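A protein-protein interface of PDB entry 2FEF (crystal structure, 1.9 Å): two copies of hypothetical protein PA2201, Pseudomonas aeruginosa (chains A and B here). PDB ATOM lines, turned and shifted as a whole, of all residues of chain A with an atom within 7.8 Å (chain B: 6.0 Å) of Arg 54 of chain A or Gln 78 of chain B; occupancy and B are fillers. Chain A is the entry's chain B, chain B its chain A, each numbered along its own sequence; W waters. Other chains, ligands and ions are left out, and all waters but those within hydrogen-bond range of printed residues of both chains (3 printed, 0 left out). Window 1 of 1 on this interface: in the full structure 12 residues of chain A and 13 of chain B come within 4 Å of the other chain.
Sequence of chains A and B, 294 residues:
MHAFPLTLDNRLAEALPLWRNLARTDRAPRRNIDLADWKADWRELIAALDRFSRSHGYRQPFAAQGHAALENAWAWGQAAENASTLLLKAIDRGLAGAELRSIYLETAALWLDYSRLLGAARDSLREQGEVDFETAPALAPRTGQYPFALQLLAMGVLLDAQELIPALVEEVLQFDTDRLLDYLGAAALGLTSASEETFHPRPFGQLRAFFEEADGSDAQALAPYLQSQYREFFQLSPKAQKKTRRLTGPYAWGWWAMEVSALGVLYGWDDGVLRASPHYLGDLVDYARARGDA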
ATOM      1  N   LEU A  12     -13.328   1.820 -30.396  1.00  0.00           N
ATOM      2  CA  LEU A  12     -13.709   0.795 -29.446  1.00  0.00           C
ATOM      3  C   LEU A  12     -15.139   0.984 -28.947  1.00  0.00           C
ATOM      4  O   LEU A  12     -15.874  -0.009 -28.772  1.00  0.00           O
ATOM      5  CB  LEU A  12     -12.721   0.763 -28.247  1.00  0.00           C
ATOM      6  CG  LEU A  12     -13.015  -0.192 -27.058  1.00  0.00           C
ATOM      7  CD1 LEU A  12     -13.125  -1.689 -27.437  1.00  0.00           C
ATOM      8  CD2 LEU A  12     -11.991   0.054 -25.936  1.00  0.00           C
ATOM      9  N   ALA A  13     -15.530   2.225 -28.662  1.00  0.00           N
ATOM     10  CA  ALA A  13     -16.866   2.446 -28.069  1.00  0.00           C
ATOM     11  C   ALA A  13     -17.972   1.986 -29.033  1.00  0.00           C
ATOM     12  O   ALA A  13     -18.968   1.414 -28.592  1.00  0.00           O
ATOM     13  CB  ALA A  13     -17.086   3.885 -27.643  1.00  0.00           C
ATOM     14  N   LEU A  16     -18.079  -2.106 -29.184  1.00  0.00           N
ATOM     15  CA  LEU A  16     -18.498  -2.895 -28.016  1.00  0.00           C
ATOM     16  C   LEU A  16     -19.903  -3.474 -28.030  1.00  0.00           C
ATOM     17  O   LEU A  16     -20.045  -4.640 -27.729  1.00  0.00           O
ATOM     18  CB  LEU A  16     -18.251  -2.154 -26.680  1.00  0.00           C
ATOM     19  CG  LEU A  16     -16.804  -2.282 -26.195  1.00  0.00           C
ATOM     20  CD1 LEU A  16     -16.516  -1.173 -25.187  1.00  0.00           C
ATOM     21  CD2 LEU A  16     -16.559  -3.643 -25.592  1.00  0.00           C
ATOM     22  N   ALA A  47     -16.793  -6.382 -20.202  1.00  0.00           N
ATOM     23  CA  ALA A  47     -16.920  -5.433 -19.063  1.00  0.00           C
ATOM     24  C   ALA A  47     -15.623  -4.655 -18.811  1.00  0.00           C
ATOM     25  O   ALA A  47     -15.666  -3.456 -18.546  1.00  0.00           O
ATOM     26  CB  ALA A  47     -17.381  -6.147 -17.772  1.00  0.00           C
ATOM     27  N   ALA A  48     -14.479  -5.320 -18.918  1.00  0.00           N
ATOM     28  CA  ALA A  48     -13.165  -4.658 -18.745  1.00  0.00           C
ATOM     29  C   ALA A  48     -12.936  -3.590 -19.842  1.00  0.00           C
ATOM     30  O   ALA A  48     -12.474  -2.483 -19.592  1.00  0.00           O
ATOM     31  CB  ALA A  48     -12.040  -5.718 -18.782  1.00  0.00           C
ATOM     32  N   LEU A  49     -13.232  -3.950 -21.074  1.00  0.00           N
ATOM     33  CA  LEU A  49     -13.065  -3.031 -22.199  1.00  0.00           C
ATOM     34  C   LEU A  49     -14.113  -1.945 -22.142  1.00  0.00           C
ATOM     35  O   LEU A  49     -13.838  -0.809 -22.503  1.00  0.00           O
ATOM     36  CB  LEU A  49     -13.161  -3.795 -23.539  1.00  0.00           C
ATOM     37  CG  LEU A  49     -11.968  -4.708 -23.847  1.00  0.00           C
ATOM     38  CD1 LEU A  49     -12.324  -5.742 -24.882  1.00  0.00           C
ATOM     39  CD2 LEU A  49     -10.795  -3.885 -24.337  1.00  0.00           C
ATOM     40  N   ASP A  50     -15.325  -2.266 -21.676  1.00  0.00           N
ATOM     41  CA  ASP A  50     -16.339  -1.219 -21.551  1.00  0.00           C
ATOM     42  C   ASP A  50     -15.914  -0.181 -20.483  1.00  0.00           C
ATOM     43  O   ASP A  50     -16.033   1.048 -20.682  1.00  0.00           O
ATOM     44  CB  ASP A  50     -17.706  -1.817 -21.199  1.00  0.00           C
ATOM     45  CG  ASP A  50     -18.837  -0.842 -21.433  1.00  0.00           C
ATOM     46  OD1 ASP A  50     -18.916   0.188 -20.727  1.00  0.00           O
ATOM     47  OD2 ASP A  50     -19.683  -1.129 -22.295  1.00  0.00           O
ATOM     48  N   ARG A  51     -15.405  -0.680 -19.363  1.00  0.00           N
ATOM     49  CA  ARG A  51     -14.893   0.155 -18.263  1.00  0.00           C
ATOM     50  C   ARG A  51     -13.789   1.081 -18.768  1.00  0.00           C
ATOM     51  O   ARG A  51     -13.769   2.302 -18.514  1.00  0.00           O
ATOM     52  CB  ARG A  51     -14.360  -0.785 -17.146  1.00  0.00           C
ATOM     53  CG  ARG A  51     -13.720  -0.095 -15.924  1.00  0.00           C
ATOM     54  CD  ARG A  51     -14.021  -0.856 -14.622  1.00  0.00           C
ATOM     55  NE  ARG A  51     -15.347  -1.478 -14.698  1.00  0.00           N
ATOM     56  CZ  ARG A  51     -16.496  -0.883 -14.366  1.00  0.00           C
ATOM     57  NH1 ARG A  51     -16.503   0.339 -13.876  1.00  0.00           N
ATOM     58  NH2 ARG A  51     -17.640  -1.538 -14.506  1.00  0.00           N
ATOM     59  N   PHE A  52     -12.843   0.481 -19.488  1.00  0.00           N
ATOM     60  CA  PHE A  52     -11.761   1.236 -20.127  1.00  0.00           C
ATOM     61  C   PHE A  52     -12.299   2.341 -21.063  1.00  0.00           C
ATOM     62  O   PHE A  52     -11.850   3.492 -21.014  1.00  0.00           O
ATOM     63  CB  PHE A  52     -10.850   0.297 -20.936  1.00  0.00           C
ATOM     64  CG  PHE A  52      -9.768   1.032 -21.725  1.00  0.00           C
ATOM     65  CD1 PHE A  52      -8.775   1.762 -21.052  1.00  0.00           C
ATOM     66  CD2 PHE A  52      -9.756   0.983 -23.116  1.00  0.00           C
ATOM     67  CE1 PHE A  52      -7.774   2.429 -21.779  1.00  0.00           C
ATOM     68  CE2 PHE A  52      -8.757   1.620 -23.843  1.00  0.00           C
ATOM     69  CZ  PHE A  52      -7.777   2.356 -23.187  1.00  0.00           C
ATOM     70  N   SER A  53     -13.281   1.990 -21.870  1.00  0.00           N
ATOM     71  CA  SER A  53     -13.904   2.952 -22.813  1.00  0.00           C
ATOM     72  C   SER A  53     -14.583   4.138 -22.110  1.00  0.00           C
ATOM     73  O   SER A  53     -14.787   5.238 -22.705  1.00  0.00           O
ATOM     74  CB  SER A  53     -14.888   2.194 -23.756  1.00  0.00           C
ATOM     75  OG  SER A  53     -16.182   2.063 -23.147  1.00  0.00           O
ATOM     76  N   ARG A  54     -14.975   3.945 -20.851  1.00  0.00           N
ATOM     77  CA  ARG A  54     -15.629   5.010 -20.097  1.00  0.00           C
ATOM     78  C   ARG A  54     -14.651   5.767 -19.212  1.00  0.00           C
ATOM     79  O   ARG A  54     -15.037   6.776 -18.611  1.00  0.00           O
ATOM     80  CB  ARG A  54     -16.794   4.471 -19.259  1.00  0.00           C
ATOM     81  CG  ARG A  54     -17.889   3.758 -20.083  1.00  0.00           C
ATOM     82  CD  ARG A  54     -18.545   4.750 -21.093  1.00  0.00           C
ATOM     83  NE  ARG A  54     -19.210   5.847 -20.377  1.00  0.00           N
ATOM     84  CZ  ARG A  54     -19.803   6.883 -20.970  1.00  0.00           C
ATOM     85  NH1 ARG A  54     -19.820   6.964 -22.290  1.00  0.00           N
ATOM     86  NH2 ARG A  54     -20.381   7.843 -20.251  1.00  0.00           N
ATOM     87  N   SER A  55     -13.400   5.291 -19.131  1.00  0.00           N
ATOM     88  CA  SER A  55     -12.356   5.951 -18.301  1.00  0.00           C
ATOM     89  C   SER A  55     -11.906   7.299 -18.860  1.00  0.00           C
ATOM     90  O   SER A  55     -11.967   7.536 -20.047  1.00  0.00           O
ATOM     91  CB  SER A  55     -11.151   4.998 -18.089  1.00  0.00           C
ATOM     92  OG  SER A  55     -10.433   4.805 -19.315  1.00  0.00           O
ATOM     93  N   HIS A  56     -11.479   8.212 -17.984  1.00  0.00           N
ATOM     94  CA  HIS A  56     -10.949   9.495 -18.421  1.00  0.00           C
ATOM     95  C   HIS A  56      -9.740   9.314 -19.331  1.00  0.00           C
ATOM     96  O   HIS A  56      -9.622  10.002 -20.321  1.00  0.00           O
ATOM     97  CB  HIS A  56     -10.549  10.350 -17.218  1.00  0.00           C
ATOM     98  CG  HIS A  56     -10.152  11.739 -17.597  1.00  0.00           C
ATOM     99  ND1 HIS A  56      -8.841  12.102 -17.809  1.00  0.00           N
ATOM    100  CD2 HIS A  56     -10.894  12.830 -17.878  1.00  0.00           C
ATOM    101  CE1 HIS A  56      -8.787  13.373 -18.167  1.00  0.00           C
ATOM    102  NE2 HIS A  56     -10.020  13.843 -18.207  1.00  0.00           N
ATOM    103  N   GLY A  57      -8.882   8.342 -19.022  1.00  0.00           N
ATOM    104  CA  GLY A  57      -7.655   8.152 -19.826  1.00  0.00           C
ATOM    105  C   GLY A  57      -7.918   7.656 -21.239  1.00  0.00           C
ATOM    106  O   GLY A  57      -7.151   7.924 -22.144  1.00  0.00           O
ATOM    107  N   TYR A  58      -9.019   6.946 -21.447  1.00  0.00           N
ATOM    108  CA  TYR A  58      -9.444   6.647 -22.821  1.00  0.00           C
ATOM    109  C   TYR A  58     -10.102   7.872 -23.507  1.00  0.00           C
ATOM    110  O   TYR A  58      -9.810   8.196 -24.649  1.00  0.00           O
ATOM    111  CB  TYR A  58     -10.413   5.473 -22.831  1.00  0.00           C
ATOM    112  CG  TYR A  58     -10.927   5.145 -24.211  1.00  0.00           C
ATOM    113  CD1 TYR A  58     -10.118   4.486 -25.129  1.00  0.00           C
ATOM    114  CD2 TYR A  58     -12.202   5.547 -24.612  1.00  0.00           C
ATOM    115  CE1 TYR A  58     -10.592   4.186 -26.422  1.00  0.00           C
ATOM    116  CE2 TYR A  58     -12.683   5.265 -25.899  1.00  0.00           C
ATOM    117  CZ  TYR A  58     -11.867   4.585 -26.786  1.00  0.00           C
ATOM    118  OH  TYR A  58     -12.341   4.327 -28.043  1.00  0.00           O
ATOM    119  N   ARG A  59     -11.016   8.525 -22.818  1.00  0.00           N
ATOM    120  CA  ARG A  59     -11.829   9.560 -23.437  1.00  0.00           C
ATOM    121  C   ARG A  59     -11.081  10.883 -23.636  1.00  0.00           C
ATOM    122  O   ARG A  59     -11.454  11.688 -24.493  1.00  0.00           O
ATOM    123  CB  ARG A  59     -13.053   9.816 -22.583  1.00  0.00           C
ATOM    124  CG  ARG A  59     -14.114   8.686 -22.642  1.00  0.00           C
ATOM    125  CD  ARG A  59     -15.445   9.309 -22.213  1.00  0.00           C
ATOM    126  NE  ARG A  59     -15.874   8.789 -20.936  1.00  0.00           N
ATOM    127  CZ  ARG A  59     -16.863   9.267 -20.176  1.00  0.00           C
ATOM    128  NH1 ARG A  59     -17.557  10.348 -20.513  1.00  0.00           N
ATOM    129  NH2 ARG A  59     -17.144   8.642 -19.051  1.00  0.00           N
ATOM    130  N   LEU B  49     -18.583  -0.644  -8.022  1.00  0.00           N
ATOM    131  CA  LEU B  49     -18.793   0.303  -6.924  1.00  0.00           C
ATOM    132  C   LEU B  49     -18.151  -0.175  -5.631  1.00  0.00           C
ATOM    133  O   LEU B  49     -17.632   0.639  -4.868  1.00  0.00           O
ATOM    134  CB  LEU B  49     -20.272   0.556  -6.709  1.00  0.00           C
ATOM    135  CG  LEU B  49     -20.848   1.423  -7.873  1.00  0.00           C
ATOM    136  CD1 LEU B  49     -22.394   1.333  -7.958  1.00  0.00           C
ATOM    137  CD2 LEU B  49     -20.349   2.861  -7.749  1.00  0.00           C
ATOM    138  N   ALA B  73     -10.091  12.512  -8.587  1.00  0.00           N
ATOM    139  CA  ALA B  73     -11.400  13.048  -8.940  1.00  0.00           C
ATOM    140  C   ALA B  73     -11.992  12.321 -10.133  1.00  0.00           C
ATOM    141  O   ALA B  73     -13.160  11.994 -10.126  1.00  0.00           O
ATOM    142  CB  ALA B  73     -11.301  14.529  -9.238  1.00  0.00           C
ATOM    143  N   TRP B  74     -11.198  12.071 -11.167  1.00  0.00           N
ATOM    144  CA  TRP B  74     -11.710  11.287 -12.318  1.00  0.00           C
ATOM    145  C   TRP B  74     -12.275   9.922 -11.936  1.00  0.00           C
ATOM    146  O   TRP B  74     -13.256   9.435 -12.541  1.00  0.00           O
ATOM    147  CB  TRP B  74     -10.617  11.142 -13.389  1.00  0.00           C
ATOM    148  CG  TRP B  74     -10.198  12.513 -13.966  1.00  0.00           C
ATOM    149  CD1 TRP B  74     -10.989  13.624 -14.102  1.00  0.00           C
ATOM    150  CD2 TRP B  74      -8.913  12.879 -14.478  1.00  0.00           C
ATOM    151  NE1 TRP B  74     -10.258  14.674 -14.643  1.00  0.00           N
ATOM    152  CE2 TRP B  74      -8.985  14.231 -14.884  1.00  0.00           C
ATOM    153  CE3 TRP B  74      -7.708  12.191 -14.639  1.00  0.00           C
ATOM    154  CZ2 TRP B  74      -7.900  14.908 -15.450  1.00  0.00           C
ATOM    155  CZ3 TRP B  74      -6.608  12.882 -15.197  1.00  0.00           C
ATOM    156  CH2 TRP B  74      -6.720  14.223 -15.597  1.00  0.00           C
ATOM    157  N   ALA B  75     -11.628   9.250 -10.988  1.00  0.00           N
ATOM    158  CA  ALA B  75     -12.132   7.945 -10.530  1.00  0.00           C
ATOM    159  C   ALA B  75     -13.518   8.077  -9.834  1.00  0.00           C
ATOM    160  O   ALA B  75     -14.414   7.248 -10.026  1.00  0.00           O
ATOM    161  CB  ALA B  75     -11.095   7.268  -9.636  1.00  0.00           C
ATOM    162  N   TRP B  76     -13.702   9.158  -9.068  1.00  0.00           N
ATOM    163  CA  TRP B  76     -14.993   9.463  -8.455  1.00  0.00           C
ATOM    164  C   TRP B  76     -16.029   9.724  -9.525  1.00  0.00           C
ATOM    165  O   TRP B  76     -17.183   9.311  -9.374  1.00  0.00           O
ATOM    166  CB  TRP B  76     -14.876  10.688  -7.517  1.00  0.00           C
ATOM    167  CG  TRP B  76     -14.295  10.394  -6.166  1.00  0.00           C
ATOM    168  CD1 TRP B  76     -12.993  10.117  -5.861  1.00  0.00           C
ATOM    169  CD2 TRP B  76     -15.018  10.340  -4.938  1.00  0.00           C
ATOM    170  NE1 TRP B  76     -12.861   9.891  -4.503  1.00  0.00           N
ATOM    171  CE2 TRP B  76     -14.098  10.009  -3.918  1.00  0.00           C
ATOM    172  CE3 TRP B  76     -16.379  10.527  -4.604  1.00  0.00           C
ATOM    173  CZ2 TRP B  76     -14.470   9.908  -2.563  1.00  0.00           C
ATOM    174  CZ3 TRP B  76     -16.761  10.402  -3.258  1.00  0.00           C
ATOM    175  CH2 TRP B  76     -15.795  10.094  -2.243  1.00  0.00           C
ATOM    176  N   GLY B  77     -15.605  10.378 -10.618  1.00  0.00           N
ATOM    177  CA  GLY B  77     -16.492  10.691 -11.750  1.00  0.00           C
ATOM    178  C   GLY B  77     -16.966   9.412 -12.418  1.00  0.00           C
ATOM    179  O   GLY B  77     -18.123   9.276 -12.742  1.00  0.00           O
ATOM    180  N   GLN B  78     -16.088   8.430 -12.542  1.00  0.00           N
ATOM    181  CA  GLN B  78     -16.542   7.146 -13.115  1.00  0.00           C
ATOM    182  C   GLN B  78     -17.448   6.348 -12.167  1.00  0.00           C
ATOM    183  O   GLN B  78     -18.396   5.704 -12.614  1.00  0.00           O
ATOM    184  CB  GLN B  78     -15.333   6.339 -13.568  1.00  0.00           C
ATOM    185  CG  GLN B  78     -15.751   5.091 -14.337  1.00  0.00           C
ATOM    186  CD  GLN B  78     -14.634   4.485 -15.194  1.00  0.00           C
ATOM    187  OE1 GLN B  78     -13.451   4.804 -15.041  1.00  0.00           O
ATOM    188  NE2 GLN B  78     -15.026   3.598 -16.124  1.00  0.00           N
ATOM    189  N   ALA B  79     -17.165   6.400 -10.854  1.00  0.00           N
ATOM    190  CA  ALA B  79     -18.074   5.805  -9.861  1.00  0.00           C
ATOM    191  C   ALA B  79     -19.452   6.467  -9.934  1.00  0.00           C
ATOM    192  O   ALA B  79     -20.480   5.777  -9.847  1.00  0.00           O
ATOM    193  CB  ALA B  79     -17.498   5.926  -8.459  1.00  0.00           C
ATOM    194  N   ALA B  80     -19.487   7.803 -10.064  1.00  0.00           N
ATOM    195  CA  ALA B  80     -20.785   8.479 -10.182  1.00  0.00           C
ATOM    196  C   ALA B  80     -21.565   7.954 -11.421  1.00  0.00           C
ATOM    197  O   ALA B  80     -22.772   7.738 -11.367  1.00  0.00           O
ATOM    198  CB  ALA B  80     -20.597  10.026 -10.253  1.00  0.00           C
ATOM    199  N   GLU B  81     -20.872   7.789 -12.548  1.00  0.00           N
ATOM    200  CA  GLU B  81     -21.509   7.245 -13.748  1.00  0.00           C
ATOM    201  C   GLU B  81     -22.014   5.847 -13.493  1.00  0.00           C
ATOM    202  O   GLU B  81     -23.101   5.483 -13.939  1.00  0.00           O
ATOM    203  CB  GLU B  81     -20.515   7.202 -14.907  1.00  0.00           C
ATOM    204  CG  GLU B  81     -20.276   8.555 -15.548  1.00  0.00           C
ATOM    205  CD  GLU B  81     -19.451   8.467 -16.834  1.00  0.00           C
ATOM    206  OE1 GLU B  81     -19.372   7.371 -17.454  1.00  0.00           O
ATOM    207  OE2 GLU B  81     -18.893   9.528 -17.199  1.00  0.00           O
ATOM    208  N   ASN B  82     -21.202   5.032 -12.814  1.00  0.00           N
ATOM    209  CA  ASN B  82     -21.637   3.657 -12.452  1.00  0.00           C
ATOM    210  C   ASN B  82     -22.917   3.651 -11.578  1.00  0.00           C
ATOM    211  O   ASN B  82     -23.805   2.814 -11.748  1.00  0.00           O
ATOM    212  CB  ASN B  82     -20.515   2.923 -11.688  1.00  0.00           C
ATOM    213  CG  ASN B  82     -19.291   2.618 -12.549  1.00  0.00           C
ATOM    214  OD1 ASN B  82     -18.230   2.274 -12.016  1.00  0.00           O
ATOM    215  ND2 ASN B  82     -19.409   2.785 -13.874  1.00  0.00           N
ATOM    216  N   ALA B  83     -22.984   4.573 -10.628  1.00  0.00           N
ATOM    217  CA  ALA B  83     -24.174   4.720  -9.780  1.00  0.00           C
ATOM    218  C   ALA B  83     -25.386   5.187 -10.623  1.00  0.00           C
ATOM    219  O   ALA B  83     -26.513   4.713 -10.412  1.00  0.00           O
ATOM    220  CB  ALA B  83     -23.902   5.733  -8.607  1.00  0.00           C
ATOM    221  N   TYR B 114     -17.971  14.013  -6.436  1.00  0.00           N
ATOM    222  CA  TYR B 114     -17.106  14.126  -7.622  1.00  0.00           C
ATOM    223  C   TYR B 114     -16.811  15.598  -7.992  1.00  0.00           C
ATOM    224  O   TYR B 114     -15.628  16.004  -8.089  1.00  0.00           O
ATOM    225  CB  TYR B 114     -17.702  13.329  -8.812  1.00  0.00           C
ATOM    226  CG  TYR B 114     -17.113  13.662 -10.162  1.00  0.00           C
ATOM    227  CD1 TYR B 114     -15.725  13.729 -10.339  1.00  0.00           C
ATOM    228  CD2 TYR B 114     -17.938  13.892 -11.290  1.00  0.00           C
ATOM    229  CE1 TYR B 114     -15.158  14.028 -11.566  1.00  0.00           C
ATOM    230  CE2 TYR B 114     -17.369  14.194 -12.520  1.00  0.00           C
ATOM    231  CZ  TYR B 114     -15.973  14.254 -12.646  1.00  0.00           C
ATOM    232  OH  TYR B 114     -15.337  14.546 -13.842  1.00  0.00           O
ATOM    233  N   PHE B 148     -26.802  11.994 -18.525  1.00  0.00           N
ATOM    234  CA  PHE B 148     -26.581  11.939 -17.065  1.00  0.00           C
ATOM    235  C   PHE B 148     -27.229  13.148 -16.405  1.00  0.00           C
ATOM    236  O   PHE B 148     -27.728  13.045 -15.281  1.00  0.00           O
ATOM    237  CB  PHE B 148     -25.084  11.896 -16.695  1.00  0.00           C
ATOM    238  CG  PHE B 148     -24.408  10.606 -17.048  1.00  0.00           C
ATOM    239  CD1 PHE B 148     -24.604   9.453 -16.268  1.00  0.00           C
ATOM    240  CD2 PHE B 148     -23.572  10.540 -18.155  1.00  0.00           C
ATOM    241  CE1 PHE B 148     -23.964   8.259 -16.599  1.00  0.00           C
ATOM    242  CE2 PHE B 148     -22.907   9.340 -18.492  1.00  0.00           C
ATOM    243  CZ  PHE B 148     -23.107   8.213 -17.711  1.00  0.00           C
ATOM    244  N   TYR B 251     -26.051   4.483 -20.601  1.00  0.00           N
ATOM    245  CA  TYR B 251     -25.562   4.466 -19.222  1.00  0.00           C
ATOM    246  C   TYR B 251     -26.459   5.182 -18.201  1.00  0.00           C
ATOM    247  O   TYR B 251     -26.269   5.006 -16.989  1.00  0.00           O
ATOM    248  CB  TYR B 251     -24.132   5.064 -19.151  1.00  0.00           C
ATOM    249  CG  TYR B 251     -23.127   4.238 -19.894  1.00  0.00           C
ATOM    250  CD1 TYR B 251     -22.514   3.129 -19.278  1.00  0.00           C
ATOM    251  CD2 TYR B 251     -22.804   4.521 -21.234  1.00  0.00           C
ATOM    252  CE1 TYR B 251     -21.593   2.353 -19.986  1.00  0.00           C
ATOM    253  CE2 TYR B 251     -21.877   3.724 -21.942  1.00  0.00           C
ATOM    254  CZ  TYR B 251     -21.295   2.651 -21.306  1.00  0.00           C
ATOM    255  OH  TYR B 251     -20.405   1.869 -21.988  1.00  0.00           O
HETATM  256  O   HOH W   1     -11.944   7.645 -15.298  1.00  0.00           O
HETATM  257  O   HOH W   2     -18.531   2.624 -24.000  1.00  0.00           O
HETATM  258  O   HOH W   3     -19.574   4.817 -17.383  1.00  0.00           O
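The side-chain amide nitrogen (NE2) of Gln 78 of chain B is in hydrogen-bond range of the backbone carbonyl oxygen (O) of Arg 51 of chain A (3.0 Å). OH of Tyr 251 of chain B lies within hydrogen-bond range of OD1 of Asp 50 of chain A (2.6 Å). OE2 of Glu 81 of chain B is in salt-bridge range of NH2 of Arg 59 of chain A. The side-chain amide oxygen (OD1) of Asn 82 of chain B sits at hydrogen-bond distance from the guanidinium group (NH1) of Arg 51 of chain A. The guanidinium group (NH2) of Arg 54 of chain A is in salt-bridge range of the side-chain carboxylate (OE1) of Glu 81 of chain B (3.0 Å).
O of Asp 50 of chain A lies within hydrogen-bond range of OG of Ser 53 of chain A. NH2 of Arg 59 of chain A sits at hydrogen-bond distance from O of Arg 54 of chain A, 2.8 Å away. ND2 of Asn 82 of chain B sits close to O of Gln 78 of chain B (3.3 Å). The backbone NH (N) of Tyr 58 of chain A sits at hydrogen-bond distance from the side-chain hydroxyl (OG) of Ser 55 of chain A, at 3.3 Å. OG of Ser 55 of chain A is in hydrogen-bond range of O of Phe 52 of chain A, at 2.6 Å.
Arg 54 of chain A touches Gln 78 of chain B. Phe 148 of chain B touches Arg 54 of chain A (CE2 to NH2, 3.4 Å). Arg 54 of chain A touches Tyr 251 of chain B (CD to CZ, 3.5 Å). CA of Ser 55 of chain A touches OE1 of Gln 78 of chain B, 3.6 Å away. His 56 of chain A touches Trp 74 of chain B.
Of the printed residues of chain A, Gln 78 of chain B touches Arg 51 (3.0 Å), Arg 54 (3.7 Å) and Ser 55 (3.6 Å). No residue of chain A comes within 4 Å of Gly 77 of chain B. No residue of chain A comes within 4 Å of Ala 79 of chain B. Printed residues of chain A within 4 Å of Asn 82 of chain B: Arg 51 (3.2 Å). Of the printed residues of chain B, Ser 55 of chain A touches Gln 78 (3.6 Å). Of the printed residues of chain A, Phe 148 of chain B touches Arg 54 (3.4 Å). Of the printed residues of chain B, Arg 51 of chain A touches Gln 78 (3.0 Å) and Asn 82 (3.2 Å). Printed residues of chain A within 4 Å of Tyr 251 of chain B: Asp 50 and Arg 54. Leu 49 of chain B touches none of the printed residues of chain A. The nearest printed residue of chain B that does not touch Arg 54 of chain A is Asn 82 of chain B (6.2 Å).
Of the 15 printed residues of chain B, 6 touch a printed residue of chain A. Hydrophobic or aromatic side chains of chain B that line the printed part of chain A: Trp 74, Phe 148 and Tyr 251. Hydrophobic or aromatic side chains of chain A within 4 Å of the printed part of chain B: His 56. Among the printed residues, Asp or Glu carboxylates within 4 Å of a Lys or Arg side-chain nitrogen of the other chain: Arg 54 of chain A with Glu 81 of chain B and Arg 59 of chain A with Glu 81 of chain B.
Position printed for both chains: 49. Of the 10 pairs that touch across the chains among the printed residues, none has its exchanged pair printed and touching as well.
Water W2 bridges the side-chain hydroxyl of Ser 53 of chain A (2.6 Å) and the side-chain hydroxyl of Tyr 251 of chain B (2.9 Å). Water W3 bridges OE1 of Glu 81 of chain B (2.6 Å) and NE of Arg 54 of chain A (3.2 Å). Water W1 bridges the backbone NH of His 56 of chain A (2.8 Å) and the side-chain amide oxygen of Gln 78 of chain B (3.2 Å).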
